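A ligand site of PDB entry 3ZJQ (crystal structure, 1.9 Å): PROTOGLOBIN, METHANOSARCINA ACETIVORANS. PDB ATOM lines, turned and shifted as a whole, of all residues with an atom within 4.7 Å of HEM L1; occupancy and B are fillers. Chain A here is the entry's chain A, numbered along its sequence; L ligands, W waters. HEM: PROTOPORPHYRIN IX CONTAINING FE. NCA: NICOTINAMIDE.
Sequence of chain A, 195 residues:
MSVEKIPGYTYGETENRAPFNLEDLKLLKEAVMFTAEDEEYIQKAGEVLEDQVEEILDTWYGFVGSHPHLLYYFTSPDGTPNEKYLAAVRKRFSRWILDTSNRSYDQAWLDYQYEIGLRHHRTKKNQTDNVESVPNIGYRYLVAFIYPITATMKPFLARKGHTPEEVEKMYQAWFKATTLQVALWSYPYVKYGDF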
ATOM      1  N   TYR A   9     -17.336   6.326  -9.693  1.00  0.00           N
ATOM      2  CA  TYR A   9     -16.399   5.752 -10.652  1.00  0.00           C
ATOM      3  C   TYR A   9     -15.342   4.901  -9.952  1.00  0.00           C
ATOM      4  O   TYR A   9     -14.481   5.436  -9.235  1.00  0.00           O
ATOM      5  CB  TYR A   9     -15.742   6.876 -11.462  1.00  0.00           C
ATOM      6  CG  TYR A   9     -14.768   6.419 -12.527  1.00  0.00           C
ATOM      7  CD1 TYR A   9     -15.228   5.847 -13.718  1.00  0.00           C
ATOM      8  CD2 TYR A   9     -13.397   6.597 -12.369  1.00  0.00           C
ATOM      9  CE1 TYR A   9     -14.333   5.430 -14.709  1.00  0.00           C
ATOM     10  CE2 TYR A   9     -12.498   6.189 -13.350  1.00  0.00           C
ATOM     11  CZ  TYR A   9     -12.971   5.620 -14.516  1.00  0.00           C
ATOM     12  OH  TYR A   9     -12.085   5.218 -15.496  1.00  0.00           O
ATOM     13  N   VAL A  64     -32.163  10.853 -25.449  1.00  0.00           N
ATOM     14  CA  VAL A  64     -32.847  10.147 -24.366  1.00  0.00           C
ATOM     15  C   VAL A  64     -33.978  11.002 -23.774  1.00  0.00           C
ATOM     16  O   VAL A  64     -35.075  10.493 -23.508  1.00  0.00           O
ATOM     17  CB  VAL A  64     -31.863   9.674 -23.251  1.00  0.00           C
ATOM     18  CG1 VAL A  64     -32.583   9.371 -21.939  1.00  0.00           C
ATOM     19  CG2 VAL A  64     -31.093   8.442 -23.716  1.00  0.00           C
ATOM     20  N   LEU A  70     -37.467   6.176 -22.814  1.00  0.00           N
ATOM     21  CA  LEU A  70     -36.032   6.073 -22.560  1.00  0.00           C
ATOM     22  C   LEU A  70     -35.630   6.895 -21.338  1.00  0.00           C
ATOM     23  O   LEU A  70     -34.967   6.365 -20.440  1.00  0.00           O
ATOM     24  CB  LEU A  70     -35.208   6.437 -23.807  1.00  0.00           C
ATOM     25  CG  LEU A  70     -35.455   5.632 -25.092  1.00  0.00           C
ATOM     26  CD1 LEU A  70     -34.651   6.221 -26.260  1.00  0.00           C
ATOM     27  CD2 LEU A  70     -35.154   4.125 -24.927  1.00  0.00           C
ATOM     28  N   TYR A  73     -35.841   5.561 -17.576  1.00  0.00           N
ATOM     29  CA  TYR A  73     -34.845   4.835 -16.776  1.00  0.00           C
ATOM     30  C   TYR A  73     -34.086   5.712 -15.771  1.00  0.00           C
ATOM     31  O   TYR A  73     -33.383   5.187 -14.908  1.00  0.00           O
ATOM     32  CB  TYR A  73     -33.920   4.007 -17.700  1.00  0.00           C
ATOM     33  CG  TYR A  73     -34.715   2.970 -18.459  1.00  0.00           C
ATOM     34  CD1 TYR A  73     -35.143   1.811 -17.813  1.00  0.00           C
ATOM     35  CD2 TYR A  73     -35.083   3.159 -19.792  1.00  0.00           C
ATOM     36  CE1 TYR A  73     -35.913   0.863 -18.470  1.00  0.00           C
ATOM     37  CE2 TYR A  73     -35.842   2.202 -20.467  1.00  0.00           C
ATOM     38  CZ  TYR A  73     -36.255   1.056 -19.789  1.00  0.00           C
ATOM     39  OH  TYR A  73     -37.016   0.091 -20.416  1.00  0.00           O
ATOM     40  N   PHE A  74     -34.242   7.029 -15.894  1.00  0.00           N
ATOM     41  CA  PHE A  74     -33.692   7.984 -14.928  1.00  0.00           C
ATOM     42  C   PHE A  74     -34.774   8.588 -14.026  1.00  0.00           C
ATOM     43  O   PHE A  74     -34.501   9.529 -13.289  1.00  0.00           O
ATOM     44  CB  PHE A  74     -32.968   9.126 -15.655  1.00  0.00           C
ATOM     45  CG  PHE A  74     -31.691   8.721 -16.335  1.00  0.00           C
ATOM     46  CD1 PHE A  74     -30.485   8.722 -15.634  1.00  0.00           C
ATOM     47  CD2 PHE A  74     -31.692   8.393 -17.690  1.00  0.00           C
ATOM     48  CE1 PHE A  74     -29.296   8.360 -16.269  1.00  0.00           C
ATOM     49  CE2 PHE A  74     -30.500   8.037 -18.333  1.00  0.00           C
ATOM     50  CZ  PHE A  74     -29.296   8.017 -17.622  1.00  0.00           C
ATOM     51  N   TYR A  85     -29.581  12.089 -10.423  1.00  0.00           N
ATOM     52  CA  TYR A  85     -29.229  10.802 -11.028  1.00  0.00           C
ATOM     53  C   TYR A  85     -28.651  11.031 -12.418  1.00  0.00           C
ATOM     54  O   TYR A  85     -27.572  10.528 -12.735  1.00  0.00           O
ATOM     55  CB  TYR A  85     -30.477   9.936 -11.105  1.00  0.00           C
ATOM     56  CG  TYR A  85     -30.302   8.479 -11.498  1.00  0.00           C
ATOM     57  CD1 TYR A  85     -29.070   7.815 -11.384  1.00  0.00           C
ATOM     58  CD2 TYR A  85     -31.397   7.750 -11.950  1.00  0.00           C
ATOM     59  CE1 TYR A  85     -28.952   6.463 -11.722  1.00  0.00           C
ATOM     60  CE2 TYR A  85     -31.288   6.410 -12.294  1.00  0.00           C
ATOM     61  CZ  TYR A  85     -30.074   5.773 -12.177  1.00  0.00           C
ATOM     62  OH  TYR A  85     -30.004   4.452 -12.519  1.00  0.00           O
ATOM     63  N   VAL A  89     -24.544  10.310 -13.310  1.00  0.00           N
ATOM     64  CA  VAL A  89     -24.241   9.352 -14.380  1.00  0.00           C
ATOM     65  C   VAL A  89     -23.488  10.027 -15.519  1.00  0.00           C
ATOM     66  O   VAL A  89     -22.552   9.433 -16.081  1.00  0.00           O
ATOM     67  CB  VAL A  89     -25.542   8.659 -14.907  1.00  0.00           C
ATOM     68  CG1 VAL A  89     -25.275   7.804 -16.135  1.00  0.00           C
ATOM     69  CG2 VAL A  89     -26.195   7.823 -13.801  1.00  0.00           C
ATOM     70  N   ARG A  92     -19.730   9.994 -15.153  1.00  0.00           N
ATOM     71  CA  ARG A  92     -19.125   8.675 -15.384  1.00  0.00           C
ATOM     72  C   ARG A  92     -19.219   8.263 -16.862  1.00  0.00           C
ATOM     73  O   ARG A  92     -18.338   7.585 -17.380  1.00  0.00           O
ATOM     74  CB  ARG A  92     -19.748   7.627 -14.466  1.00  0.00           C
ATOM     75  CG  ARG A  92     -19.611   7.964 -12.982  1.00  0.00           C
ATOM     76  CD  ARG A  92     -19.919   6.788 -12.083  1.00  0.00           C
ATOM     77  NE  ARG A  92     -21.321   6.376 -12.153  1.00  0.00           N
ATOM     78  CZ  ARG A  92     -22.294   6.863 -11.382  1.00  0.00           C
ATOM     79  NH1 ARG A  92     -22.037   7.805 -10.484  1.00  0.00           N
ATOM     80  NH2 ARG A  92     -23.530   6.412 -11.519  1.00  0.00           N
ATOM     81  N   PHE A  93     -20.298   8.694 -17.522  1.00  0.00           N
ATOM     82  CA  PHE A  93     -20.504   8.501 -18.962  1.00  0.00           C
ATOM     83  C   PHE A  93     -19.444   9.273 -19.760  1.00  0.00           C
ATOM     84  O   PHE A  93     -18.894   8.765 -20.742  1.00  0.00           O
ATOM     85  CB  PHE A  93     -21.919   8.992 -19.326  1.00  0.00           C
ATOM     86  CG  PHE A  93     -22.411   8.529 -20.683  1.00  0.00           C
ATOM     87  CD1 PHE A  93     -21.968   7.348 -21.257  1.00  0.00           C
ATOM     88  CD2 PHE A  93     -23.367   9.278 -21.350  1.00  0.00           C
ATOM     89  CE1 PHE A  93     -22.450   6.926 -22.492  1.00  0.00           C
ATOM     90  CE2 PHE A  93     -23.862   8.862 -22.584  1.00  0.00           C
ATOM     91  CZ  PHE A  93     -23.405   7.675 -23.159  1.00  0.00           C
ATOM     92  N   TRP A  96     -16.234   7.463 -19.418  1.00  0.00           N
ATOM     93  CA  TRP A  96     -16.288   6.270 -20.236  1.00  0.00           C
ATOM     94  C   TRP A  96     -15.790   6.531 -21.657  1.00  0.00           C
ATOM     95  O   TRP A  96     -15.076   5.723 -22.229  1.00  0.00           O
ATOM     96  CB  TRP A  96     -17.711   5.702 -20.286  1.00  0.00           C
ATOM     97  CG  TRP A  96     -17.883   4.606 -21.299  1.00  0.00           C
ATOM     98  CD1 TRP A  96     -17.515   3.303 -21.151  1.00  0.00           C
ATOM     99  CD2 TRP A  96     -18.455   4.717 -22.613  1.00  0.00           C
ATOM    100  NE1 TRP A  96     -17.819   2.593 -22.291  1.00  0.00           N
ATOM    101  CE2 TRP A  96     -18.399   3.437 -23.201  1.00  0.00           C
ATOM    102  CE3 TRP A  96     -19.010   5.774 -23.353  1.00  0.00           C
ATOM    103  CZ2 TRP A  96     -18.875   3.179 -24.498  1.00  0.00           C
ATOM    104  CZ3 TRP A  96     -19.493   5.517 -24.638  1.00  0.00           C
ATOM    105  CH2 TRP A  96     -19.412   4.221 -25.203  1.00  0.00           C
ATOM    106  N   TYR A 112     -14.188  -3.753 -15.159  1.00  0.00           N
ATOM    107  CA  TYR A 112     -15.098  -2.602 -15.165  1.00  0.00           C
ATOM    108  C   TYR A 112     -16.237  -2.759 -16.185  1.00  0.00           C
ATOM    109  O   TYR A 112     -17.323  -2.228 -15.971  1.00  0.00           O
ATOM    110  CB  TYR A 112     -14.381  -1.266 -15.350  1.00  0.00           C
ATOM    111  CG  TYR A 112     -15.153  -0.132 -14.723  1.00  0.00           C
ATOM    112  CD1 TYR A 112     -15.394  -0.122 -13.353  1.00  0.00           C
ATOM    113  CD2 TYR A 112     -15.680   0.903 -15.487  1.00  0.00           C
ATOM    114  CE1 TYR A 112     -16.125   0.904 -12.748  1.00  0.00           C
ATOM    115  CE2 TYR A 112     -16.419   1.948 -14.896  1.00  0.00           C
ATOM    116  CZ  TYR A 112     -16.625   1.933 -13.521  1.00  0.00           C
ATOM    117  OH  TYR A 112     -17.352   2.917 -12.910  1.00  0.00           O
ATOM    118  N   ILE A 116     -20.134  -2.178 -15.390  1.00  0.00           N
ATOM    119  CA  ILE A 116     -21.073  -1.326 -16.140  1.00  0.00           C
ATOM    120  C   ILE A 116     -22.325  -2.124 -16.533  1.00  0.00           C
ATOM    121  O   ILE A 116     -23.452  -1.616 -16.452  1.00  0.00           O
ATOM    122  CB  ILE A 116     -20.413  -0.656 -17.362  1.00  0.00           C
ATOM    123  CG1 ILE A 116     -19.288   0.282 -16.922  1.00  0.00           C
ATOM    124  CG2 ILE A 116     -21.460   0.112 -18.185  1.00  0.00           C
ATOM    125  CD1 ILE A 116     -18.337   0.732 -18.045  1.00  0.00           C
ATOM    126  N   ARG A 119     -24.510  -2.461 -13.571  1.00  0.00           N
ATOM    127  CA  ARG A 119     -25.154  -1.204 -13.202  1.00  0.00           C
ATOM    128  C   ARG A 119     -26.373  -0.848 -14.052  1.00  0.00           C
ATOM    129  O   ARG A 119     -27.244  -0.127 -13.588  1.00  0.00           O
ATOM    130  CB  ARG A 119     -24.151  -0.044 -13.183  1.00  0.00           C
ATOM    131  CG  ARG A 119     -23.215  -0.077 -11.979  1.00  0.00           C
ATOM    132  CD  ARG A 119     -22.157   1.011 -12.043  1.00  0.00           C
ATOM    133  NE  ARG A 119     -21.198   0.842 -10.950  1.00  0.00           N
ATOM    134  CZ  ARG A 119     -20.267   1.729 -10.602  1.00  0.00           C
ATOM    135  NH1 ARG A 119     -20.154   2.886 -11.234  1.00  0.00           N
ATOM    136  NH2 ARG A 119     -19.460   1.451  -9.580  1.00  0.00           N
ATOM    137  N   HIS A 120     -26.421  -1.350 -15.286  1.00  0.00           N
ATOM    138  CA  HIS A 120     -27.614  -1.198 -16.124  1.00  0.00           C
ATOM    139  C   HIS A 120     -28.663  -2.218 -15.706  1.00  0.00           C
ATOM    140  O   HIS A 120     -29.861  -1.955 -15.784  1.00  0.00           O
ATOM    141  CB  HIS A 120     -27.290  -1.350 -17.629  1.00  0.00           C
ATOM    142  CG  HIS A 120     -26.592  -0.177 -18.228  1.00  0.00           C
ATOM    143  ND1 HIS A 120     -25.219  -0.031 -18.194  1.00  0.00           N
ATOM    144  CD2 HIS A 120     -27.070   0.917 -18.866  1.00  0.00           C
ATOM    145  CE1 HIS A 120     -24.888   1.100 -18.777  1.00  0.00           C
ATOM    146  NE2 HIS A 120     -25.983   1.702 -19.198  1.00  0.00           N
ATOM    147  N   LYS A 124     -27.186  -4.108  -9.884  1.00  0.00           N
ATOM    148  CA  LYS A 124     -26.590  -2.933  -9.247  1.00  0.00           C
ATOM    149  C   LYS A 124     -27.207  -1.584  -9.632  1.00  0.00           C
ATOM    150  O   LYS A 124     -26.765  -0.553  -9.112  1.00  0.00           O
ATOM    151  CB  LYS A 124     -25.074  -2.889  -9.497  1.00  0.00           C
ATOM    152  CG  LYS A 124     -24.281  -3.988  -8.785  1.00  0.00           C
ATOM    153  CD  LYS A 124     -22.804  -3.625  -8.645  1.00  0.00           C
ATOM    154  CE  LYS A 124     -22.586  -2.641  -7.490  1.00  0.00           C
ATOM    155  NZ  LYS A 124     -21.176  -2.135  -7.417  1.00  0.00           N
ATOM    156  N   LYS A 125     -28.203  -1.574 -10.519  1.00  0.00           N
ATOM    157  CA  LYS A 125     -28.816  -0.298 -10.910  1.00  0.00           C
ATOM    158  C   LYS A 125     -29.328   0.444  -9.681  1.00  0.00           C
ATOM    159  O   LYS A 125     -29.912  -0.168  -8.795  1.00  0.00           O
ATOM    160  CB  LYS A 125     -29.957  -0.475 -11.920  1.00  0.00           C
ATOM    161  CG  LYS A 125     -30.393   0.865 -12.561  1.00  0.00           C
ATOM    162  CD  LYS A 125     -31.566   0.728 -13.521  1.00  0.00           C
ATOM    163  CE  LYS A 125     -31.954   2.111 -14.092  1.00  0.00           C
ATOM    164  NZ  LYS A 125     -32.624   2.983 -13.058  1.00  0.00           N
ATOM    165  N   ASN A 126     -29.061   1.757  -9.632  1.00  0.00           N
ATOM    166  CA  ASN A 126     -29.522   2.664  -8.570  1.00  0.00           C
ATOM    167  C   ASN A 126     -28.740   2.629  -7.247  1.00  0.00           C
ATOM    168  O   ASN A 126     -29.009   3.429  -6.345  1.00  0.00           O
ATOM    169  CB  ASN A 126     -30.973   2.385  -8.156  1.00  0.00           C
ATOM    170  CG  ASN A 126     -31.931   2.385  -9.328  1.00  0.00           C
ATOM    171  OD1 ASN A 126     -31.834   3.228 -10.226  1.00  0.00           O
ATOM    172  ND2 ASN A 126     -32.852   1.425  -9.348  1.00  0.00           N
ATOM    173  N   THR A 128     -25.156   2.815  -7.047  1.00  0.00           N
ATOM    174  CA  THR A 128     -23.981   3.676  -7.113  1.00  0.00           C
ATOM    175  C   THR A 128     -24.254   5.101  -6.633  1.00  0.00           C
ATOM    176  O   THR A 128     -23.443   5.677  -5.899  1.00  0.00           O
ATOM    177  CB  THR A 128     -23.375   3.674  -8.529  1.00  0.00           C
ATOM    178  OG1 THR A 128     -23.006   2.338  -8.894  1.00  0.00           O
ATOM    179  CG2 THR A 128     -22.141   4.559  -8.607  1.00  0.00           C
ATOM    180  N   ILE A 137     -32.879  -1.866 -16.579  1.00  0.00           N
ATOM    181  CA  ILE A 137     -32.950  -1.387 -17.959  1.00  0.00           C
ATOM    182  C   ILE A 137     -33.032  -2.579 -18.897  1.00  0.00           C
ATOM    183  O   ILE A 137     -32.075  -3.346 -19.034  1.00  0.00           O
ATOM    184  CB  ILE A 137     -31.751  -0.496 -18.363  1.00  0.00           C
ATOM    185  CG1 ILE A 137     -31.653   0.731 -17.443  1.00  0.00           C
ATOM    186  CG2 ILE A 137     -31.881  -0.033 -19.821  1.00  0.00           C
ATOM    187  CD1 ILE A 137     -30.321   1.461 -17.508  1.00  0.00           C
ATOM    188  N   TYR A 141     -32.805  -2.433 -25.135  1.00  0.00           N
ATOM    189  CA  TYR A 141     -32.422  -1.036 -25.354  1.00  0.00           C
ATOM    190  C   TYR A 141     -30.914  -0.790 -25.347  1.00  0.00           C
ATOM    191  O   TYR A 141     -30.444   0.118 -26.017  1.00  0.00           O
ATOM    192  CB  TYR A 141     -33.138  -0.095 -24.361  1.00  0.00           C
ATOM    193  CG  TYR A 141     -34.632  -0.019 -24.580  1.00  0.00           C
ATOM    194  CD1 TYR A 141     -35.152   0.427 -25.788  1.00  0.00           C
ATOM    195  CD2 TYR A 141     -35.524  -0.419 -23.584  1.00  0.00           C
ATOM    196  CE1 TYR A 141     -36.518   0.491 -26.008  1.00  0.00           C
ATOM    197  CE2 TYR A 141     -36.908  -0.361 -23.790  1.00  0.00           C
ATOM    198  CZ  TYR A 141     -37.392   0.094 -25.004  1.00  0.00           C
ATOM    199  OH  TYR A 141     -38.745   0.152 -25.225  1.00  0.00           O
ATOM    200  N   LEU A 142     -30.179  -1.594 -24.591  1.00  0.00           N
ATOM    201  CA  LEU A 142     -28.705  -1.540 -24.655  1.00  0.00           C
ATOM    202  C   LEU A 142     -28.198  -1.906 -26.055  1.00  0.00           C
ATOM    203  O   LEU A 142     -27.312  -1.240 -26.597  1.00  0.00           O
ATOM    204  CB  LEU A 142     -28.090  -2.469 -23.613  1.00  0.00           C
ATOM    205  CG  LEU A 142     -27.761  -1.924 -22.232  1.00  0.00           C
ATOM    206  CD1 LEU A 142     -29.015  -1.662 -21.420  1.00  0.00           C
ATOM    207  CD2 LEU A 142     -26.838  -2.888 -21.503  1.00  0.00           C
ATOM    208  N   PHE A 145     -29.163   0.882 -28.495  1.00  0.00           N
ATOM    209  CA  PHE A 145     -28.335   2.076 -28.348  1.00  0.00           C
ATOM    210  C   PHE A 145     -26.971   1.993 -29.031  1.00  0.00           C
ATOM    211  O   PHE A 145     -26.289   3.012 -29.162  1.00  0.00           O
ATOM    212  CB  PHE A 145     -28.157   2.432 -26.860  1.00  0.00           C
ATOM    213  CG  PHE A 145     -29.213   3.364 -26.325  1.00  0.00           C
ATOM    214  CD1 PHE A 145     -30.534   3.298 -26.766  1.00  0.00           C
ATOM    215  CD2 PHE A 145     -28.883   4.302 -25.347  1.00  0.00           C
ATOM    216  CE1 PHE A 145     -31.514   4.163 -26.247  1.00  0.00           C
ATOM    217  CE2 PHE A 145     -29.844   5.155 -24.817  1.00  0.00           C
ATOM    218  CZ  PHE A 145     -31.158   5.088 -25.270  1.00  0.00           C
ATOM    219  N   ILE A 146     -26.578   0.793 -29.461  1.00  0.00           N
ATOM    220  CA  ILE A 146     -25.369   0.648 -30.285  1.00  0.00           C
ATOM    221  C   ILE A 146     -25.465   1.591 -31.476  1.00  0.00           C
ATOM    222  O   ILE A 146     -24.484   2.257 -31.829  1.00  0.00           O
ATOM    223  CB  ILE A 146     -25.114  -0.814 -30.763  1.00  0.00           C
ATOM    224  CG1 ILE A 146     -24.730  -1.728 -29.589  1.00  0.00           C
ATOM    225  CG2 ILE A 146     -24.020  -0.847 -31.839  1.00  0.00           C
ATOM    226  CD1 ILE A 146     -24.675  -3.240 -29.952  1.00  0.00           C
ATOM    227  N   ILE A 149     -25.320   5.536 -30.231  1.00  0.00           N
ATOM    228  CA  ILE A 149     -23.982   5.783 -29.637  1.00  0.00           C
ATOM    229  C   ILE A 149     -22.866   5.762 -30.694  1.00  0.00           C
ATOM    230  O   ILE A 149     -21.910   6.528 -30.595  1.00  0.00           O
ATOM    231  CB  ILE A 149     -23.666   4.809 -28.445  1.00  0.00           C
ATOM    232  CG1 ILE A 149     -24.644   5.023 -27.277  1.00  0.00           C
ATOM    233  CG2 ILE A 149     -22.205   4.979 -27.955  1.00  0.00           C
ATOM    234  CD1 ILE A 149     -24.648   6.424 -26.673  1.00  0.00           C
ATOM    235  N   THR A 178     -17.790   0.020 -29.260  1.00  0.00           N
ATOM    236  CA  THR A 178     -19.153   0.132 -28.717  1.00  0.00           C
ATOM    237  C   THR A 178     -19.862  -1.230 -28.758  1.00  0.00           C
ATOM    238  O   THR A 178     -20.379  -1.703 -27.738  1.00  0.00           O
ATOM    239  CB  THR A 178     -19.965   1.199 -29.493  1.00  0.00           C
ATOM    240  OG1 THR A 178     -19.313   2.469 -29.360  1.00  0.00           O
ATOM    241  CG2 THR A 178     -21.393   1.322 -28.938  1.00  0.00           C
ATOM    242  N   VAL A 182     -21.049  -3.522 -25.410  1.00  0.00           N
ATOM    243  CA  VAL A 182     -22.444  -3.927 -25.194  1.00  0.00           C
ATOM    244  C   VAL A 182     -22.581  -5.447 -25.168  1.00  0.00           C
ATOM    245  O   VAL A 182     -23.378  -5.987 -24.398  1.00  0.00           O
ATOM    246  CB  VAL A 182     -23.416  -3.261 -26.217  1.00  0.00           C
ATOM    247  CG1 VAL A 182     -24.821  -3.839 -26.102  1.00  0.00           C
ATOM    248  CG2 VAL A 182     -23.470  -1.753 -25.983  1.00  0.00           C
ATOM    249  N   TRP A 185     -21.603  -6.479 -21.763  1.00  0.00           N
ATOM    250  CA  TRP A 185     -22.588  -6.055 -20.774  1.00  0.00           C
ATOM    251  C   TRP A 185     -23.833  -6.941 -20.743  1.00  0.00           C
ATOM    252  O   TRP A 185     -24.633  -6.840 -19.813  1.00  0.00           O
ATOM    253  CB  TRP A 185     -22.994  -4.582 -20.968  1.00  0.00           C
ATOM    254  CG  TRP A 185     -21.850  -3.596 -20.992  1.00  0.00           C
ATOM    255  CD1 TRP A 185     -20.540  -3.830 -20.679  1.00  0.00           C
ATOM    256  CD2 TRP A 185     -21.943  -2.211 -21.322  1.00  0.00           C
ATOM    257  NE1 TRP A 185     -19.808  -2.675 -20.838  1.00  0.00           N
ATOM    258  CE2 TRP A 185     -20.647  -1.667 -21.218  1.00  0.00           C
ATOM    259  CE3 TRP A 185     -23.000  -1.359 -21.716  1.00  0.00           C
ATOM    260  CZ2 TRP A 185     -20.362  -0.322 -21.494  1.00  0.00           C
ATOM    261  CZ3 TRP A 185     -22.718  -0.034 -21.983  1.00  0.00           C
ATOM    262  CH2 TRP A 185     -21.413   0.477 -21.863  1.00  0.00           C
HETATM  263  CHA HEM L   1     -24.962   4.164 -16.825  1.00  0.00           C
HETATM  264  CHB HEM L   1     -23.048   3.972 -21.284  1.00  0.00           C
HETATM  265  CHC HEM L   1     -27.222   1.971 -22.722  1.00  0.00           C
HETATM  266  CHD HEM L   1     -29.254   4.475 -19.107  1.00  0.00           C
HETATM  267  C1A HEM L   1     -24.026   4.220 -17.842  1.00  0.00           C
HETATM  268  C2A HEM L   1     -22.599   4.503 -17.737  1.00  0.00           C
HETATM  269  C3A HEM L   1     -22.084   4.426 -18.976  1.00  0.00           C
HETATM  270  C4A HEM L   1     -23.144   4.117 -19.905  1.00  0.00           C
HETATM  271  CMA HEM L   1     -20.612   4.653 -19.374  1.00  0.00           C
HETATM  272  CAA HEM L   1     -21.827   4.801 -16.430  1.00  0.00           C
HETATM  273  CBA HEM L   1     -21.049   3.566 -15.994  1.00  0.00           C
HETATM  274  CGA HEM L   1     -20.374   3.825 -14.663  1.00  0.00           C
HETATM  275  O1A HEM L   1     -19.147   4.092 -14.648  1.00  0.00           O
HETATM  276  O2A HEM L   1     -21.069   3.743 -13.618  1.00  0.00           O
HETATM  277  C1B HEM L   1     -23.982   3.328 -22.069  1.00  0.00           C
HETATM  278  C2B HEM L   1     -23.788   2.816 -23.413  1.00  0.00           C
HETATM  279  C3B HEM L   1     -24.932   2.239 -23.819  1.00  0.00           C
HETATM  280  C4B HEM L   1     -25.897   2.391 -22.743  1.00  0.00           C
HETATM  281  CMB HEM L   1     -22.456   2.919 -24.180  1.00  0.00           C
HETATM  282  CAB HEM L   1     -25.243   1.535 -25.166  1.00  0.00           C
HETATM  283  CBB HEM L   1     -24.514   1.645 -26.284  1.00  0.00           C
HETATM  284  C1C HEM L   1     -28.190   2.579 -21.952  1.00  0.00           C
HETATM  285  C2C HEM L   1     -29.628   2.656 -22.189  1.00  0.00           C
HETATM  286  C3C HEM L   1     -30.176   3.361 -21.186  1.00  0.00           C
HETATM  287  C4C HEM L   1     -29.131   3.753 -20.274  1.00  0.00           C
HETATM  288  CMC HEM L   1     -30.404   2.031 -23.368  1.00  0.00           C
HETATM  289  CAC HEM L   1     -31.675   3.698 -21.039  1.00  0.00           C
HETATM  290  CBC HEM L   1     -32.030   4.978 -20.968  1.00  0.00           C
HETATM  291  C1D HEM L   1     -28.364   4.458 -18.059  1.00  0.00           C
HETATM  292  C2D HEM L   1     -28.652   4.628 -16.649  1.00  0.00           C
HETATM  293  C3D HEM L   1     -27.304   4.532 -15.951  1.00  0.00           C
HETATM  294  C4D HEM L   1     -26.321   4.301 -16.993  1.00  0.00           C
HETATM  295  CMD HEM L   1     -30.030   4.857 -15.982  1.00  0.00           C
HETATM  296  CAD HEM L   1     -27.011   4.606 -14.444  1.00  0.00           C
HETATM  297  CBD HEM L   1     -27.123   3.162 -13.967  1.00  0.00           C
HETATM  298  CGD HEM L   1     -26.869   3.064 -12.488  1.00  0.00           C
HETATM  299  O1D HEM L   1     -27.814   3.297 -11.691  1.00  0.00           O
HETATM  300  O2D HEM L   1     -25.711   2.739 -12.118  1.00  0.00           O
HETATM  301  NA  HEM L   1     -24.311   4.001 -19.169  1.00  0.00           N
HETATM  302  NB  HEM L   1     -25.273   3.055 -21.699  1.00  0.00           N
HETATM  303  NC  HEM L   1     -27.945   3.260 -20.776  1.00  0.00           N
HETATM  304  ND  HEM L   1     -27.002   4.261 -18.205  1.00  0.00           N
HETATM  305 FE   HEM L   1     -26.124   3.638 -19.950  1.00  0.00          FE
HETATM  306  N1  NCA L   2     -26.272   5.692 -20.574  1.00  0.00           N
HETATM  307  C2  NCA L   2     -26.722   6.088 -21.770  1.00  0.00           C
HETATM  308  C3  NCA L   2     -26.986   7.434 -21.979  1.00  0.00           C
HETATM  309  C4  NCA L   2     -26.777   8.361 -20.961  1.00  0.00           C
HETATM  310  C5  NCA L   2     -26.307   7.922 -19.725  1.00  0.00           C
HETATM  311  C6  NCA L   2     -26.062   6.575 -19.566  1.00  0.00           C
HETATM  312  C7  NCA L   2     -27.480   7.914 -23.313  1.00  0.00           C
HETATM  313  O7  NCA L   2     -27.427   7.161 -24.273  1.00  0.00           O
HETATM  314  N7  NCA L   2     -27.968   9.144 -23.406  1.00  0.00           N
HETATM  315  O   HOH W   1     -17.571   4.964 -16.614  1.00  0.00           O
HETATM  316  O   HOH W   2     -23.793   4.014 -13.529  1.00  0.00           O
HETATM  317  O   HOH W   3     -26.861   4.823  -9.363  1.00  0.00           O
HETATM  318  O   HOH W   4     -25.437   1.617  -9.715  1.00  0.00           O
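FE of HEM L1 is bound by NE2 of His 120, at 2.1 Å. The side-chain hydroxyl of Tyr 85 is in hydrogen-bond range of an oxygen (O1D) of HEM L1 (2.6 Å). An oxygen (O2A) of HEM L1 is in salt-bridge range of the guanidinium group (NH1) of Arg 119. An oxygen (O1A) of HEM L1 is in hydrogen-bond range of the side-chain hydroxyl (OH) of Tyr 112 (2.8 Å). An oxygen (O1D) of HEM L1 is in hydrogen-bond range of the backbone NH (N) of Asn 126 (2.9 Å). The guanidinium group of Arg 92 lies within salt-bridge range of an oxygen (O2A) of HEM L1 (3.0 Å).
A nitrogen (N1) of NCA L2 is bound to an iron atom (FE) of HEM L1.
The backbone carbonyl oxygen (O) of His 120 is in hydrogen-bond range of the backbone NH (N) of Ile 137 (3.1 Å). A ring nitrogen (ND1) of His 120 is in hydrogen-bond range of the backbone carbonyl oxygen of Ile 116 (2.9 Å). The side-chain hydroxyl (OH) of Tyr 85 is in hydrogen-bond range of the side-chain amide oxygen (OD1) of Asn 126. The side-chain hydroxyl (OH) of Tyr 85 lies within hydrogen-bond range of the side-chain amino group (NZ) of Lys 125 (3.1 Å). The guanidinium group (NH1) of Arg 119 is in hydrogen-bond range of the side-chain hydroxyl (OH) of Tyr 112 (3.3 Å). NE of Arg 119 is in hydrogen-bond range of OG1 of Thr 128 (3.1 Å). The side-chain amide oxygen (OD1) of Asn 126 is in hydrogen-bond range of the side-chain amino group (NZ) of Lys 125, at 3.0 Å. The backbone carbonyl oxygen of Tyr 73 lies within hydrogen-bond range of the side-chain amino group of Lys 125.
Residues that only touch HEM L1: Leu 70, Tyr 73, Phe 74, Val 89, Phe 93, Trp 96, Ile 116, Lys 125, Ile 137, Tyr 141, Leu 142, Phe 145, Ile 146, Ile 149, Val 182 and Trp 185. Within 4 Å of HEM L1: Leu 70, Tyr 73, Phe 74, Tyr 85, Val 89, Arg 92, Phe 93, Trp 96, Tyr 112, Ile 116, Arg 119, His 120, Lys 125, Asn 126, Ile 137, Tyr 141, Leu 142, Phe 145, Ile 146, Ile 149, Val 182 and Trp 185.
Water W1 bridges an oxygen (O1A) of HEM L1 and the backbone carbonyl oxygen (O) of Arg 92. Water W4 lies within hydrogen-bond range of O of Lys 124 (2.6 Å), OG1 of Thr 128 (2.7 Å) and O2D of HEM L1 (2.7 Å). Water W2 lies within hydrogen-bond range of O2D of HEM L1 (2.7 Å) and NH2 of Arg 92 (3.1 Å).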
